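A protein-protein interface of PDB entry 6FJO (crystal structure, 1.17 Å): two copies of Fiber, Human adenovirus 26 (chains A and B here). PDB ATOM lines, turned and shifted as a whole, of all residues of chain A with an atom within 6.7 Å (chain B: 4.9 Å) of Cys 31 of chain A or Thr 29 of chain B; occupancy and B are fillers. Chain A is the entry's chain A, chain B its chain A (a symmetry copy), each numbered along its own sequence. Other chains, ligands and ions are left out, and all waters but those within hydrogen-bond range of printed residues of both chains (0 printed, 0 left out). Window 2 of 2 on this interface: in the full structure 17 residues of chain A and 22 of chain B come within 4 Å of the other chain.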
ATOM      1  N   ARG A   2      -1.234  11.240 -26.478  1.00  0.00           N
ATOM      2  CA  ARG A   2      -0.997  12.449 -25.813  1.00  0.00           C
ATOM      3  C   ARG A   2       0.424  12.613 -25.398  1.00  0.00           C
ATOM      4  O   ARG A   2       0.724  13.662 -24.924  1.00  0.00           O
ATOM      5  CB  ARG A   2      -1.971  12.698 -24.677  1.00  0.00           C
ATOM      6  CG  ARG A   2      -3.420  12.909 -25.180  1.00  0.00           C
ATOM      7  CD  ARG A   2      -3.721  14.253 -25.861  1.00  0.00           C
ATOM      8  NE  ARG A   2      -3.982  15.296 -24.832  1.00  0.00           N
ATOM      9  CZ  ARG A   2      -4.891  16.299 -24.903  1.00  0.00           C
ATOM     10  NH1 ARG A   2      -4.981  17.157 -23.881  1.00  0.00           N
ATOM     11  NH2 ARG A   2      -5.663  16.501 -25.990  1.00  0.00           N
ATOM     12  N   THR A  29       4.187  16.007 -23.363  1.00  0.00           N
ATOM     13  CA  THR A  29       2.920  15.557 -23.029  1.00  0.00           C
ATOM     14  C   THR A  29       1.877  16.637 -23.254  1.00  0.00           C
ATOM     15  O   THR A  29       2.009  17.745 -22.706  1.00  0.00           O
ATOM     16  CB  THR A  29       2.812  15.033 -21.581  1.00  0.00           C
ATOM     17  OG1 THR A  29       3.819  14.002 -21.440  1.00  0.00           O
ATOM     18  CG2 THR A  29       1.483  14.546 -21.291  1.00  0.00           C
ATOM     19  N   LYS A  30       0.872  16.373 -24.028  1.00  0.00           N
ATOM     20  CA  LYS A  30      -0.176  17.357 -24.306  1.00  0.00           C
ATOM     21  C   LYS A  30      -1.113  17.487 -23.154  1.00  0.00           C
ATOM     22  O   LYS A  30      -1.728  16.496 -22.758  1.00  0.00           O
ATOM     23  CB  LYS A  30      -0.933  16.905 -25.550  1.00  0.00           C
ATOM     24  CG  LYS A  30      -2.157  17.662 -25.956  1.00  0.00           C
ATOM     25  CD  LYS A  30      -1.782  18.957 -26.556  1.00  0.00           C
ATOM     26  CE  LYS A  30      -2.944  19.428 -27.438  1.00  0.00           C
ATOM     27  NZ  LYS A  30      -2.696  20.815 -27.826  1.00  0.00           N
ATOM     28  N   CYS A  31      -1.326  18.742 -22.762  1.00  0.00           N
ATOM     29  CA  CYS A  31      -2.123  19.133 -21.657  1.00  0.00           C
ATOM     30  C   CYS A  31      -3.061  20.303 -22.139  1.00  0.00           C
ATOM     31  O   CYS A  31      -2.828  21.463 -21.789  1.00  0.00           O
ATOM     32  CB  CYS A  31      -1.157  19.556 -20.533  1.00  0.00           C
ATOM     33  SG  CYS A  31      -0.156  18.211 -19.795  1.00  0.00           S
ATOM     34  N   GLY A  32      -4.021  20.042 -23.024  1.00  0.00           N
ATOM     35  CA  GLY A  32      -4.800  21.094 -23.577  1.00  0.00           C
ATOM     36  C   GLY A  32      -3.997  22.091 -24.373  1.00  0.00           C
ATOM     37  O   GLY A  32      -3.239  21.747 -25.307  1.00  0.00           O
ATOM     38  N   SER A  33      -4.069  23.352 -23.986  1.00  0.00           N
ATOM     39  CA  SER A  33      -3.424  24.452 -24.693  1.00  0.00           C
ATOM     40  C   SER A  33      -1.907  24.521 -24.411  1.00  0.00           C
ATOM     41  O   SER A  33      -1.205  25.442 -24.883  1.00  0.00           O
ATOM     42  CB  SER A  33      -4.128  25.758 -24.282  1.00  0.00           C
ATOM     43  OG  SER A  33      -3.352  26.889 -24.677  1.00  0.00           O
ATOM     44  N   GLN A  34      -1.374  23.644 -23.545  1.00  0.00           N
ATOM     45  CA  GLN A  34       0.075  23.594 -23.317  1.00  0.00           C
ATOM     46  C   GLN A  34       0.621  22.152 -23.524  1.00  0.00           C
ATOM     47  O   GLN A  34      -0.138  21.187 -23.315  1.00  0.00           O
ATOM     48  CB  GLN A  34       0.453  24.079 -21.933  1.00  0.00           C
ATOM     49  CG  GLN A  34       0.217  25.585 -21.771  1.00  0.00           C
ATOM     50  CD  GLN A  34       0.543  26.021 -20.343  1.00  0.00           C
ATOM     51  OE1 GLN A  34       1.712  26.027 -19.957  1.00  0.00           O
ATOM     52  NE2 GLN A  34      -0.465  26.344 -19.581  1.00  0.00           N
ATOM     53  N   VAL A  35       1.834  22.069 -23.888  1.00  0.00           N
ATOM     54  CA  VAL A  35       2.636  20.853 -23.726  1.00  0.00           C
ATOM     55  C   VAL A  35       3.414  21.022 -22.438  1.00  0.00           C
ATOM     56  O   VAL A  35       4.060  22.045 -22.207  1.00  0.00           O
ATOM     57  CB  VAL A  35       3.531  20.624 -24.916  1.00  0.00           C
ATOM     58  CG1 VAL A  35       4.749  19.749 -24.606  1.00  0.00           C
ATOM     59  CG2 VAL A  35       2.732  20.018 -26.036  1.00  0.00           C
ATOM     60  N   LEU A  36       3.480  19.930 -21.644  1.00  0.00           N
ATOM     61  CA  LEU A  36       4.403  19.753 -20.522  1.00  0.00           C
ATOM     62  C   LEU A  36       5.599  18.975 -21.038  1.00  0.00           C
ATOM     63  O   LEU A  36       5.432  17.806 -21.461  1.00  0.00           O
ATOM     64  CB  LEU A  36       3.671  19.031 -19.404  1.00  0.00           C
ATOM     65  CG  LEU A  36       4.434  18.714 -18.153  1.00  0.00           C
ATOM     66  CD1 LEU A  36       4.875  20.018 -17.462  1.00  0.00           C
ATOM     67  CD2 LEU A  36       3.664  17.839 -17.200  1.00  0.00           C
ATOM     68  N   THR A 182       0.550  25.651 -27.325  1.00  0.00           N
ATOM     69  CA  THR A 182       0.508  24.872 -28.560  1.00  0.00           C
ATOM     70  C   THR A 182      -0.302  25.532 -29.666  1.00  0.00           C
ATOM     71  O   THR A 182      -1.224  26.344 -29.422  1.00  0.00           O
ATOM     72  CB  THR A 182      -0.026  23.475 -28.347  1.00  0.00           C
ATOM     73  OG1 THR A 182      -1.359  23.536 -27.900  1.00  0.00           O
ATOM     74  CG2 THR A 182       0.757  22.754 -27.292  1.00  0.00           C
ATOM     75  N   ARG B   2     -10.744  24.476 -20.394  1.00  0.00           N
ATOM     76  CA  ARG B   2      -9.682  24.125 -19.552  1.00  0.00           C
ATOM     77  C   ARG B   2      -8.530  25.063 -19.651  1.00  0.00           C
ATOM     78  O   ARG B   2      -7.634  24.892 -18.887  1.00  0.00           O
ATOM     79  CB  ARG B   2      -9.267  22.673 -19.699  1.00  0.00           C
ATOM     80  CG  ARG B   2     -10.369  21.696 -19.220  1.00  0.00           C
ATOM     81  CD  ARG B   2     -10.573  21.585 -17.701  1.00  0.00           C
ATOM     82  NE  ARG B   2      -9.568  20.654 -17.120  1.00  0.00           N
ATOM     83  CZ  ARG B   2      -9.765  19.770 -16.112  1.00  0.00           C
ATOM     84  NH1 ARG B   2      -8.736  19.015 -15.710  1.00  0.00           N
ATOM     85  NH2 ARG B   2     -10.939  19.667 -15.459  1.00  0.00           N
ATOM     86  N   THR B   3      -8.621  26.159 -20.404  1.00  0.00           N
ATOM     87  CA  THR B   3      -7.618  27.226 -20.398  1.00  0.00           C
ATOM     88  C   THR B   3      -8.197  28.633 -20.247  1.00  0.00           C
ATOM     89  O   THR B   3      -9.109  29.029 -20.972  1.00  0.00           O
ATOM     90  CB  THR B   3      -6.678  27.154 -21.615  1.00  0.00           C
ATOM     91  OG1 THR B   3      -5.823  25.951 -21.479  1.00  0.00           O
ATOM     92  CG2 THR B   3      -5.816  28.312 -21.776  1.00  0.00           C
ATOM     93  N   THR B  27      -1.053  32.169 -19.513  1.00  0.00           N
ATOM     94  CA  THR B  27      -1.924  31.079 -19.786  1.00  0.00           C
ATOM     95  C   THR B  27      -2.018  30.162 -18.587  1.00  0.00           C
ATOM     96  O   THR B  27      -0.977  29.812 -17.990  1.00  0.00           O
ATOM     97  CB  THR B  27      -1.356  30.234 -20.967  1.00  0.00           C
ATOM     98  OG1 THR B  27      -1.110  31.141 -22.070  1.00  0.00           O
ATOM     99  CG2 THR B  27      -2.169  29.098 -21.376  1.00  0.00           C
ATOM    100  N   LEU B  28      -3.231  29.860 -18.176  1.00  0.00           N
ATOM    101  CA  LEU B  28      -3.537  28.946 -17.040  1.00  0.00           C
ATOM    102  C   LEU B  28      -4.292  27.803 -17.576  1.00  0.00           C
ATOM    103  O   LEU B  28      -5.441  27.960 -18.042  1.00  0.00           O
ATOM    104  CB  LEU B  28      -4.348  29.727 -15.977  1.00  0.00           C
ATOM    105  CG  LEU B  28      -3.750  30.977 -15.412  1.00  0.00           C
ATOM    106  CD1 LEU B  28      -4.735  31.657 -14.456  1.00  0.00           C
ATOM    107  CD2 LEU B  28      -2.426  30.781 -14.732  1.00  0.00           C
ATOM    108  N   THR B  29      -3.720  26.572 -17.549  1.00  0.00           N
ATOM    109  CA  THR B  29      -4.322  25.413 -18.011  1.00  0.00           C
ATOM    110  C   THR B  29      -4.682  24.486 -16.864  1.00  0.00           C
ATOM    111  O   THR B  29      -3.802  24.126 -16.064  1.00  0.00           O
ATOM    112  CB  THR B  29      -3.472  24.645 -19.045  1.00  0.00           C
ATOM    113  OG1 THR B  29      -3.178  25.578 -20.112  1.00  0.00           O
ATOM    114  CG2 THR B  29      -4.154  23.463 -19.520  1.00  0.00           C
ATOM    115  N   LYS B  30      -5.914  24.100 -16.746  1.00  0.00           N
ATOM    116  CA  LYS B  30      -6.350  23.212 -15.666  1.00  0.00           C
ATOM    117  C   LYS B  30      -5.946  21.802 -15.931  1.00  0.00           C
ATOM    118  O   LYS B  30      -6.335  21.242 -16.958  1.00  0.00           O
ATOM    119  CB  LYS B  30      -7.867  23.311 -15.555  1.00  0.00           C
ATOM    120  CG  LYS B  30      -8.578  22.381 -14.624  1.00  0.00           C
ATOM    121  CD  LYS B  30      -8.368  22.799 -13.224  1.00  0.00           C
ATOM    122  CE  LYS B  30      -9.506  22.218 -12.378  1.00  0.00           C
ATOM    123  NZ  LYS B  30      -9.172  22.403 -10.967  1.00  0.00           N
ATOM    124  N   CYS B  31      -5.322  21.212 -14.914  1.00  0.00           N
ATOM    125  CA  CYS B  31      -4.783  19.901 -14.928  1.00  0.00           C
ATOM    126  C   CYS B  31      -5.249  19.182 -13.607  1.00  0.00           C
ATOM    127  O   CYS B  31      -4.444  19.002 -12.688  1.00  0.00           O
ATOM    128  CB  CYS B  31      -3.253  20.044 -15.033  1.00  0.00           C
ATOM    129  SG  CYS B  31      -2.621  20.708 -16.620  1.00  0.00           S
ATOM    130  N   GLN B  34      -4.203  20.784 -10.095  1.00  0.00           N
ATOM    131  CA  GLN B  34      -3.253  21.880 -10.321  1.00  0.00           C
ATOM    132  C   GLN B  34      -3.621  22.680 -11.604  1.00  0.00           C
ATOM    133  O   GLN B  34      -4.221  22.094 -12.524  1.00  0.00           O
ATOM    134  CB  GLN B  34      -1.826  21.385 -10.432  1.00  0.00           C
ATOM    135  CG  GLN B  34      -1.298  20.856  -9.092  1.00  0.00           C
ATOM    136  CD  GLN B  34       0.116  20.303  -9.262  1.00  0.00           C
ATOM    137  OE1 GLN B  34       1.053  21.073  -9.479  1.00  0.00           O
ATOM    138  NE2 GLN B  34       0.254  19.008  -9.195  1.00  0.00           N
ATOM    139  N   VAL B  35      -3.260  23.896 -11.617  1.00  0.00           N
ATOM    140  CA  VAL B  35      -3.128  24.678 -12.849  1.00  0.00           C
ATOM    141  C   VAL B  35      -1.666  24.619 -13.239  1.00  0.00           C
ATOM    142  O   VAL B  35      -0.774  24.869 -12.427  1.00  0.00           O
ATOM    143  CB  VAL B  35      -3.619  26.089 -12.658  1.00  0.00           C
ATOM    144  CG1 VAL B  35      -3.026  27.084 -13.660  1.00  0.00           C
ATOM    145  CG2 VAL B  35      -5.121  26.113 -12.734  1.00  0.00           C
ATOM    146  N   LEU B  36      -1.416  24.434 -14.555  1.00  0.00           N
ATOM    147  CA  LEU B  36      -0.123  24.640 -15.208  1.00  0.00           C
ATOM    148  C   LEU B  36      -0.133  26.037 -15.801  1.00  0.00           C
ATOM    149  O   LEU B  36      -0.960  26.312 -16.704  1.00  0.00           O
ATOM    150  CB  LEU B  36       0.066  23.558 -16.257  1.00  0.00           C
ATOM    151  CG  LEU B  36       1.319  23.586 -17.079  1.00  0.00           C
ATOM    152  CD1 LEU B  36       2.546  23.376 -16.173  1.00  0.00           C
ATOM    153  CD2 LEU B  36       1.308  22.585 -18.203  1.00  0.00           C
ATOM    154  N   PHE B 101      -9.911  27.347 -11.381  1.00  0.00           N
ATOM    155  CA  PHE B 101      -8.608  27.921 -11.707  1.00  0.00           C
ATOM    156  C   PHE B 101      -8.012  28.715 -10.586  1.00  0.00           C
ATOM    157  O   PHE B 101      -6.893  29.184 -10.687  1.00  0.00           O
ATOM    158  CB  PHE B 101      -8.691  28.833 -12.929  1.00  0.00           C
ATOM    159  CG  PHE B 101      -9.030  28.105 -14.212  1.00  0.00           C
ATOM    160  CD1 PHE B 101     -10.296  27.729 -14.503  1.00  0.00           C
ATOM    161  CD2 PHE B 101      -8.001  27.797 -15.131  1.00  0.00           C
ATOM    162  CE1 PHE B 101     -10.605  27.040 -15.675  1.00  0.00           C
ATOM    163  CE2 PHE B 101      -8.316  27.143 -16.298  1.00  0.00           C
ATOM    164  CZ  PHE B 101      -9.551  26.800 -16.571  1.00  0.00           C
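Of the 10 printed residues of chain A, 3 touch a printed residue of chain B.
Printed residues of chain A that touch a printed residue of chain B: Cys 31, Ser 33 and Gln 34.
Of the 11 printed residues of chain B, 4 touch a printed residue of chain A.
Printed residues of chain B that touch a printed residue of chain A: Thr 3, Thr 27, Thr 29 and Leu 36.
Of the printed residues of chain B, Cys 31 of chain A touches Thr 29.
Of the printed residues of chain A, Thr 29 of chain B touches Cys 31 (3.3 Å) and Gln 34 (2.9 Å).
Of the printed residues of chain B, Ser 33 of chain A touches Thr 3 (3.3 Å).
Printed residues of chain A within 4 Å of Thr 27 of chain B: Gln 34.
Of the printed residues of chain A, Thr 3 of chain B touches Ser 33 (3.3 Å).
Val 35 of chain A touches none of the printed residues of chain B.
Thr 182 of chain A touches none of the printed residues of chain B.
The nearest printed residue of chain B that does not touch Cys 31 of chain A is Cys 31 of chain B (4.3 Å).
The nearest printed residue of chain A that does not touch Thr 29 of chain B is Ser 33 of chain A (4.3 Å).
NE2 of Gln 34 of chain A is in hydrogen-bond range of OG1 of Thr 29 of chain B, 2.9 Å away.
NE2 of Gln 34 of chain A sits at hydrogen-bond distance from O of Leu 36 of chain B (2.9 Å).
Cys 31 of chain A touches Thr 29 of chain B (O to CG2, 3.3 Å).
Thr 3 of chain B touches Ser 33 of chain A (OG1 to CB, 3.3 Å).
NE2 of Gln 34 of chain A touches CG2 of Thr 27 of chain B, at 3.7 Å.
Cys 31 of chain A touches Thr 29 of chain B, but with the chains exchanged Thr 29 of chain A does not touch Cys 31 of chain B (8.2 Å).
Gln 34 of chain A touches Thr 29 of chain B, but with the chains exchanged Thr 29 of chain A does not touch Gln 34 of chain B (12.7 Å).
Gln 34 of chain A touches Leu 36 of chain B, but with the chains exchanged Leu 36 of chain A does not touch Gln 34 of chain B (8.8 Å).
Positions printed for both chains: 2, 29, 30, 31, 34, 35 and 36.
The side-chain hydroxyl (OG1) of Thr 29 of chain B sits at hydrogen-bond distance from the side-chain hydroxyl (OG1) of Thr 3 of chain B.
O of Thr 29 of chain B sits at hydrogen-bond distance from N of Leu 36 of chain B (2.8 Å).
N of Thr 182 of chain A lies within hydrogen-bond range of O of Ser 33 of chain A (3.0 Å).
The side-chain sulfur of Cys 31 of chain B sits at hydrogen-bond distance from the backbone carbonyl oxygen of Thr 29 of chain B (3.7 Å).
The backbone carbonyl oxygen (O) of Thr 29 of chain A is in hydrogen-bond range of the side-chain sulfur (SG) of Cys 31 of chain A, at 3.7 Å.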
